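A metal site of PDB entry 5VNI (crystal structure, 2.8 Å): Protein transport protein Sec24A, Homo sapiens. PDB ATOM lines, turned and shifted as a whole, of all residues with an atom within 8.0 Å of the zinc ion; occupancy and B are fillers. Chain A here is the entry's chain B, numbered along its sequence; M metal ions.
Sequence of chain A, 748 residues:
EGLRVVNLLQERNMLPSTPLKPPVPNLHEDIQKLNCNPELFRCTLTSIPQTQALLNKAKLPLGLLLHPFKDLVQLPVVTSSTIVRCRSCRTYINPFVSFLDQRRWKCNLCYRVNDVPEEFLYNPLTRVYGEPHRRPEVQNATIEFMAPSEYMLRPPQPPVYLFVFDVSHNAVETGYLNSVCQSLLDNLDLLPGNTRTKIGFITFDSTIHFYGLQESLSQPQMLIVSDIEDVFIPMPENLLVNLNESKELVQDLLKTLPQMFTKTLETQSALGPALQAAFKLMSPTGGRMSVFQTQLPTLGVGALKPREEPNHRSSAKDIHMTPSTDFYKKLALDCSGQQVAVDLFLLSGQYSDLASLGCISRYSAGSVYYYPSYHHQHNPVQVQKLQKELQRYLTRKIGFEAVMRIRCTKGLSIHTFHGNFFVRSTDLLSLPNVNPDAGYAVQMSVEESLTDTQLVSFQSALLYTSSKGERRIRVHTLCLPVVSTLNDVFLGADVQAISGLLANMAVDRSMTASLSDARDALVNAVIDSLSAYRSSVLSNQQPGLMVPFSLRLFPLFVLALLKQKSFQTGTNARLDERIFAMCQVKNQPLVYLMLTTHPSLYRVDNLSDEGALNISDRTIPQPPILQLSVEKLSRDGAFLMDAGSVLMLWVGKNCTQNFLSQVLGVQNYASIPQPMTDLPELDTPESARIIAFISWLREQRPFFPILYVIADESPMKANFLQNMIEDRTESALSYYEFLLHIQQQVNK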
ATOM      1  N   ARG A  85     -19.819 -33.713  -7.603  1.00  0.00           N
ATOM      2  CA  ARG A  85     -19.551 -32.843  -8.743  1.00  0.00           C
ATOM      3  C   ARG A  85     -19.342 -31.415  -8.245  1.00  0.00           C
ATOM      4  O   ARG A  85     -19.908 -31.014  -7.231  1.00  0.00           O
ATOM      5  CB  ARG A  85     -20.685 -32.875  -9.770  1.00  0.00           C
ATOM      6  CG  ARG A  85     -20.952 -34.249 -10.350  1.00  0.00           C
ATOM      7  CD  ARG A  85     -22.140 -34.242 -11.302  1.00  0.00           C
ATOM      8  NE  ARG A  85     -21.811 -33.624 -12.577  1.00  0.00           N
ATOM      9  CZ  ARG A  85     -22.687 -33.470 -13.573  1.00  0.00           C
ATOM     10  NH1 ARG A  85     -23.938 -33.882 -13.429  1.00  0.00           N
ATOM     11  NH2 ARG A  85     -22.310 -32.896 -14.710  1.00  0.00           N
ATOM     12  N   CYS A  86     -18.520 -30.665  -8.977  1.00  0.00           N
ATOM     13  CA  CYS A  86     -18.253 -29.276  -8.627  1.00  0.00           C
ATOM     14  C   CYS A  86     -19.537 -28.465  -8.720  1.00  0.00           C
ATOM     15  O   CYS A  86     -20.282 -28.563  -9.697  1.00  0.00           O
ATOM     16  CB  CYS A  86     -17.189 -28.703  -9.548  1.00  0.00           C
ATOM     17  SG  CYS A  86     -16.899 -26.931  -9.326  1.00  0.00           S
ATOM     18  N   ARG A  87     -19.794 -27.646  -7.695  1.00  0.00           N
ATOM     19  CA  ARG A  87     -21.022 -26.865  -7.634  1.00  0.00           C
ATOM     20  C   ARG A  87     -21.097 -25.775  -8.693  1.00  0.00           C
ATOM     21  O   ARG A  87     -22.160 -25.167  -8.853  1.00  0.00           O
ATOM     22  CB  ARG A  87     -21.182 -26.240  -6.247  1.00  0.00           C
ATOM     23  CG  ARG A  87     -21.553 -27.220  -5.148  1.00  0.00           C
ATOM     24  CD  ARG A  87     -21.690 -26.500  -3.811  1.00  0.00           C
ATOM     25  NE  ARG A  87     -22.102 -27.390  -2.732  1.00  0.00           N
ATOM     26  CZ  ARG A  87     -22.217 -27.019  -1.465  1.00  0.00           C
ATOM     27  NH1 ARG A  87     -21.953 -25.769  -1.108  1.00  0.00           N
ATOM     28  NH2 ARG A  87     -22.604 -27.888  -0.548  1.00  0.00           N
ATOM     29  N   SER A  88     -20.015 -25.511  -9.423  1.00  0.00           N
ATOM     30  CA  SER A  88     -20.019 -24.454 -10.429  1.00  0.00           C
ATOM     31  C   SER A  88     -20.195 -25.018 -11.838  1.00  0.00           C
ATOM     32  O   SER A  88     -21.225 -24.780 -12.476  1.00  0.00           O
ATOM     33  CB  SER A  88     -18.736 -23.629 -10.355  1.00  0.00           C
ATOM     34  OG  SER A  88     -18.798 -22.682  -9.309  1.00  0.00           O
ATOM     35  N   CYS A  89     -19.195 -25.749 -12.333  1.00  0.00           N
ATOM     36  CA  CYS A  89     -19.197 -26.258 -13.697  1.00  0.00           C
ATOM     37  C   CYS A  89     -19.600 -27.724 -13.796  1.00  0.00           C
ATOM     38  O   CYS A  89     -19.452 -28.325 -14.856  1.00  0.00           O
ATOM     39  CB  CYS A  89     -17.827 -26.050 -14.338  1.00  0.00           C
ATOM     40  SG  CYS A  89     -16.477 -26.939 -13.524  1.00  0.00           S
ATOM     41  N   ARG A  90     -20.090 -28.305 -12.697  1.00  0.00           N
ATOM     42  CA  ARG A  90     -20.599 -29.682 -12.677  1.00  0.00           C
ATOM     43  C   ARG A  90     -19.537 -30.706 -13.068  1.00  0.00           C
ATOM     44  O   ARG A  90     -19.858 -31.786 -13.563  1.00  0.00           O
ATOM     45  CB  ARG A  90     -21.829 -29.819 -13.587  1.00  0.00           C
ATOM     46  CG  ARG A  90     -22.939 -28.818 -13.312  1.00  0.00           C
ATOM     47  CD  ARG A  90     -23.352 -28.804 -11.849  1.00  0.00           C
ATOM     48  NE  ARG A  90     -23.529 -30.150 -11.313  1.00  0.00           N
ATOM     49  CZ  ARG A  90     -24.620 -30.888 -11.473  1.00  0.00           C
ATOM     50  NH1 ARG A  90     -25.646 -30.422 -12.165  1.00  0.00           N
ATOM     51  NH2 ARG A  90     -24.686 -32.106 -10.938  1.00  0.00           N
ATOM     52  N   THR A  91     -18.270 -30.381 -12.838  1.00  0.00           N
ATOM     53  CA  THR A  91     -17.189 -31.311 -13.124  1.00  0.00           C
ATOM     54  C   THR A  91     -17.141 -32.398 -12.054  1.00  0.00           C
ATOM     55  O   THR A  91     -17.121 -32.101 -10.861  1.00  0.00           O
ATOM     56  CB  THR A  91     -15.856 -30.579 -13.201  1.00  0.00           C
ATOM     57  OG1 THR A  91     -15.876 -29.647 -14.295  1.00  0.00           O
ATOM     58  CG2 THR A  91     -14.717 -31.563 -13.406  1.00  0.00           C
ATOM     59  N   TYR A  92     -17.117 -33.657 -12.499  1.00  0.00           N
ATOM     60  CA  TYR A  92     -17.022 -34.769 -11.577  1.00  0.00           C
ATOM     61  C   TYR A  92     -15.653 -34.767 -10.881  1.00  0.00           C
ATOM     62  O   TYR A  92     -14.639 -34.368 -11.467  1.00  0.00           O
ATOM     63  CB  TYR A  92     -17.223 -36.094 -12.306  1.00  0.00           C
ATOM     64  CG  TYR A  92     -18.551 -36.196 -13.035  1.00  0.00           C
ATOM     65  CD1 TYR A  92     -18.727 -35.624 -14.289  1.00  0.00           C
ATOM     66  CD2 TYR A  92     -19.622 -36.868 -12.463  1.00  0.00           C
ATOM     67  CE1 TYR A  92     -19.938 -35.714 -14.943  1.00  0.00           C
ATOM     68  CE2 TYR A  92     -20.836 -36.966 -13.121  1.00  0.00           C
ATOM     69  CZ  TYR A  92     -20.985 -36.384 -14.366  1.00  0.00           C
ATOM     70  OH  TYR A  92     -22.187 -36.475 -15.023  1.00  0.00           O
ATOM     71  N   ASN A  94     -12.242 -35.781  -9.775  1.00  0.00           N
ATOM     72  CA  ASN A  94     -11.271 -36.527 -10.566  1.00  0.00           C
ATOM     73  C   ASN A  94      -9.936 -36.566  -9.834  1.00  0.00           C
ATOM     74  O   ASN A  94      -9.706 -35.786  -8.905  1.00  0.00           O
ATOM     75  CB  ASN A  94     -11.104 -35.890 -11.955  1.00  0.00           C
ATOM     76  CG  ASN A  94     -10.737 -34.429 -11.895  1.00  0.00           C
ATOM     77  OD1 ASN A  94      -9.560 -34.067 -11.936  1.00  0.00           O
ATOM     78  ND2 ASN A  94     -11.737 -33.560 -11.800  1.00  0.00           N
ATOM     79  N   TRP A 105     -12.088 -29.406  -1.578  1.00  0.00           N
ATOM     80  CA  TRP A 105     -11.274 -29.659  -2.746  1.00  0.00           C
ATOM     81  C   TRP A 105     -11.452 -28.544  -3.770  1.00  0.00           C
ATOM     82  O   TRP A 105     -12.535 -27.984  -3.914  1.00  0.00           O
ATOM     83  CB  TRP A 105     -11.618 -31.018  -3.387  1.00  0.00           C
ATOM     84  CG  TRP A 105     -13.039 -31.146  -3.875  1.00  0.00           C
ATOM     85  CD1 TRP A 105     -14.132 -31.409  -3.116  1.00  0.00           C
ATOM     86  CD2 TRP A 105     -13.499 -31.036  -5.233  1.00  0.00           C
ATOM     87  NE1 TRP A 105     -15.255 -31.469  -3.913  1.00  0.00           N
ATOM     88  CE2 TRP A 105     -14.892 -31.237  -5.211  1.00  0.00           C
ATOM     89  CE3 TRP A 105     -12.865 -30.782  -6.453  1.00  0.00           C
ATOM     90  CZ2 TRP A 105     -15.671 -31.195  -6.372  1.00  0.00           C
ATOM     91  CZ3 TRP A 105     -13.639 -30.736  -7.601  1.00  0.00           C
ATOM     92  CH2 TRP A 105     -15.022 -30.942  -7.550  1.00  0.00           C
ATOM     93  N   LYS A 106     -10.361 -28.231  -4.464  1.00  0.00           N
ATOM     94  CA  LYS A 106     -10.369 -27.206  -5.498  1.00  0.00           C
ATOM     95  C   LYS A 106     -10.623 -27.846  -6.865  1.00  0.00           C
ATOM     96  O   LYS A 106      -9.948 -28.799  -7.245  1.00  0.00           O
ATOM     97  CB  LYS A 106      -9.042 -26.441  -5.519  1.00  0.00           C
ATOM     98  CG  LYS A 106      -8.869 -25.527  -6.721  1.00  0.00           C
ATOM     99  CD  LYS A 106      -7.538 -24.797  -6.692  1.00  0.00           C
ATOM    100  CE  LYS A 106      -7.486 -23.784  -5.564  1.00  0.00           C
ATOM    101  NZ  LYS A 106      -6.203 -23.031  -5.553  1.00  0.00           N
ATOM    102  N   CYS A 107     -11.598 -27.301  -7.587  1.00  0.00           N
ATOM    103  CA  CYS A 107     -11.931 -27.824  -8.911  1.00  0.00           C
ATOM    104  C   CYS A 107     -10.820 -27.473  -9.899  1.00  0.00           C
ATOM    105  O   CYS A 107     -10.440 -26.304 -10.029  1.00  0.00           O
ATOM    106  CB  CYS A 107     -13.260 -27.256  -9.387  1.00  0.00           C
ATOM    107  SG  CYS A 107     -13.766 -27.820 -11.033  1.00  0.00           S
ATOM    108  N   ASN A 108     -10.319 -28.488 -10.602  1.00  0.00           N
ATOM    109  CA  ASN A 108      -9.227 -28.277 -11.544  1.00  0.00           C
ATOM    110  C   ASN A 108      -9.659 -27.585 -12.826  1.00  0.00           C
ATOM    111  O   ASN A 108      -8.791 -27.259 -13.655  1.00  0.00           O
ATOM    112  CB  ASN A 108      -8.548 -29.611 -11.864  1.00  0.00           C
ATOM    113  CG  ASN A 108      -9.559 -30.728 -12.070  1.00  0.00           C
ATOM    114  OD1 ASN A 108     -10.643 -30.724 -11.475  1.00  0.00           O
ATOM    115  ND2 ASN A 108      -9.211 -31.697 -12.900  1.00  0.00           N
ATOM    116  N   LEU A 109     -10.952 -27.359 -13.028  1.00  0.00           N
ATOM    117  CA  LEU A 109     -11.458 -26.725 -14.235  1.00  0.00           C
ATOM    118  C   LEU A 109     -11.941 -25.295 -14.022  1.00  0.00           C
ATOM    119  O   LEU A 109     -11.681 -24.444 -14.871  1.00  0.00           O
ATOM    120  CB  LEU A 109     -12.591 -27.555 -14.838  1.00  0.00           C
ATOM    121  CG  LEU A 109     -12.190 -28.729 -15.727  1.00  0.00           C
ATOM    122  CD1 LEU A 109     -11.734 -29.934 -14.903  1.00  0.00           C
ATOM    123  CD2 LEU A 109     -13.324 -29.114 -16.652  1.00  0.00           C
ATOM    124  N   CYS A 110     -12.640 -25.019 -12.927  1.00  0.00           N
ATOM    125  CA  CYS A 110     -13.124 -23.669 -12.638  1.00  0.00           C
ATOM    126  C   CYS A 110     -12.546 -23.078 -11.369  1.00  0.00           C
ATOM    127  O   CYS A 110     -12.955 -21.977 -10.982  1.00  0.00           O
ATOM    128  CB  CYS A 110     -14.657 -23.662 -12.561  1.00  0.00           C
ATOM    129  SG  CYS A 110     -15.330 -24.561 -11.152  1.00  0.00           S
ATOM    130  N   TYR A 111     -11.643 -23.782 -10.675  1.00  0.00           N
ATOM    131  CA  TYR A 111     -10.872 -23.258  -9.554  1.00  0.00           C
ATOM    132  C   TYR A 111     -11.732 -22.949  -8.328  1.00  0.00           C
ATOM    133  O   TYR A 111     -11.191 -22.532  -7.299  1.00  0.00           O
ATOM    134  CB  TYR A 111     -10.109 -21.999  -9.972  1.00  0.00           C
ATOM    135  CG  TYR A 111      -9.237 -22.196 -11.200  1.00  0.00           C
ATOM    136  CD1 TYR A 111      -8.548 -23.386 -11.395  1.00  0.00           C
ATOM    137  CD2 TYR A 111      -9.124 -21.205 -12.161  1.00  0.00           C
ATOM    138  CE1 TYR A 111      -7.763 -23.573 -12.516  1.00  0.00           C
ATOM    139  CE2 TYR A 111      -8.346 -21.383 -13.275  1.00  0.00           C
ATOM    140  CZ  TYR A 111      -7.661 -22.567 -13.454  1.00  0.00           C
ATOM    141  OH  TYR A 111      -6.883 -22.731 -14.572  1.00  0.00           O
ATOM    142  N   ARG A 112     -13.038 -23.161  -8.412  1.00  0.00           N
ATOM    143  CA  ARG A 112     -13.892 -22.948  -7.253  1.00  0.00           C
ATOM    144  C   ARG A 112     -13.679 -24.053  -6.224  1.00  0.00           C
ATOM    145  O   ARG A 112     -13.532 -25.233  -6.569  1.00  0.00           O
ATOM    146  CB  ARG A 112     -15.362 -22.890  -7.669  1.00  0.00           C
ATOM    147  CG  ARG A 112     -16.306 -23.411  -6.591  1.00  0.00           C
ATOM    148  CD  ARG A 112     -17.572 -22.576  -6.452  1.00  0.00           C
ATOM    149  NE  ARG A 112     -18.365 -23.022  -5.310  1.00  0.00           N
ATOM    150  CZ  ARG A 112     -19.645 -22.697  -5.117  1.00  0.00           C
ATOM    151  NH1 ARG A 112     -20.273 -21.911  -5.986  1.00  0.00           N
ATOM    152  NH2 ARG A 112     -20.285 -23.151  -4.053  1.00  0.00           N
ATOM    153  N   VAL A 113     -13.662 -23.677  -4.950  1.00  0.00           N
ATOM    154  CA  VAL A 113     -13.505 -24.622  -3.861  1.00  0.00           C
ATOM    155  C   VAL A 113     -14.862 -25.218  -3.522  1.00  0.00           C
ATOM    156  O   VAL A 113     -15.862 -24.502  -3.440  1.00  0.00           O
ATOM    157  CB  VAL A 113     -12.861 -23.948  -2.639  1.00  0.00           C
ATOM    158  CG1 VAL A 113     -12.431 -24.995  -1.624  1.00  0.00           C
ATOM    159  CG2 VAL A 113     -11.683 -23.088  -3.069  1.00  0.00           C
ATOM    160  N   ASN A 114     -14.893 -26.534  -3.315  1.00  0.00           N
ATOM    161  CA  ASN A 114     -16.111 -27.253  -2.971  1.00  0.00           C
ATOM    162  C   ASN A 114     -15.958 -27.924  -1.609  1.00  0.00           C
ATOM    163  O   ASN A 114     -14.878 -27.965  -1.033  1.00  0.00           O
ATOM    164  CB  ASN A 114     -16.455 -28.302  -4.035  1.00  0.00           C
ATOM    165  CG  ASN A 114     -17.057 -27.686  -5.292  1.00  0.00           C
ATOM    166  OD1 ASN A 114     -18.273 -27.656  -5.462  1.00  0.00           O
ATOM    167  ND2 ASN A 114     -16.196 -27.180  -6.162  1.00  0.00           N
ATOM    168  N   ARG A 407     -15.715 -31.260 -21.023  1.00  0.00           N
ATOM    169  CA  ARG A 407     -15.347 -30.104 -20.204  1.00  0.00           C
ATOM    170  C   ARG A 407     -13.831 -29.951 -20.174  1.00  0.00           C
ATOM    171  O   ARG A 407     -13.103 -30.947 -20.073  1.00  0.00           O
ATOM    172  CB  ARG A 407     -15.889 -30.239 -18.782  1.00  0.00           C
ATOM    173  CG  ARG A 407     -17.402 -30.211 -18.688  1.00  0.00           C
ATOM    174  CD  ARG A 407     -17.858 -30.247 -17.239  1.00  0.00           C
ATOM    175  NE  ARG A 407     -19.308 -30.162 -17.111  1.00  0.00           N
ATOM    176  CZ  ARG A 407     -20.125 -31.210 -17.116  1.00  0.00           C
ATOM    177  NH1 ARG A 407     -19.626 -32.437 -17.235  1.00  0.00           N
ATOM    178  NH2 ARG A 407     -21.432 -31.045 -17.002  1.00  0.00           N
HETATM  179 ZN    ZN M   1     -15.799 -26.772 -11.346  1.00  0.00          ZN
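The side-chain hydroxyl (OG1) of Thr 91 sits close to the side-chain sulfur (SG) of Cys 89 (2.9 Å). NE of Arg 407 is in hydrogen-bond range of O of Cys 89, at 2.9 Å. N of Cys 86 lies within hydrogen-bond range of O of Thr 91 (2.8 Å). The backbone NH (N) of Ser 88 lies close to the side-chain sulfur (SG) of Cys 86 (3.4 Å). The side-chain amide nitrogen of Asn 114 lies close to the side-chain sulfur of Cys 86 (3.3 Å). The side-chain sulfur (SG) of Cys 107 lies close to the backbone NH (N) of Leu 109 (3.5 Å). The backbone carbonyl oxygen (O) of Arg 112 is in hydrogen-bond range of the backbone NH (N) of Cys 107 (3.0 Å).
Four residues have an atom within 4 Å of the zinc ion: Cys 86, Cys 89, Cys 107 and Cys 110. The nearest printed residue that does not touch the zinc ion is Thr 91 (4.1 Å).
SG of Cys 110 binds the zinc ion (2.3 Å). The zinc ion is bound by the side-chain sulfur (SG) of Cys 89 (2.3 Å). The side-chain sulfur (SG) of Cys 86 binds the zinc ion (2.3 Å). The zinc ion is bound by SG of Cys 107 (2.3 Å). The zinc ion has four donor atoms within binding distance.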
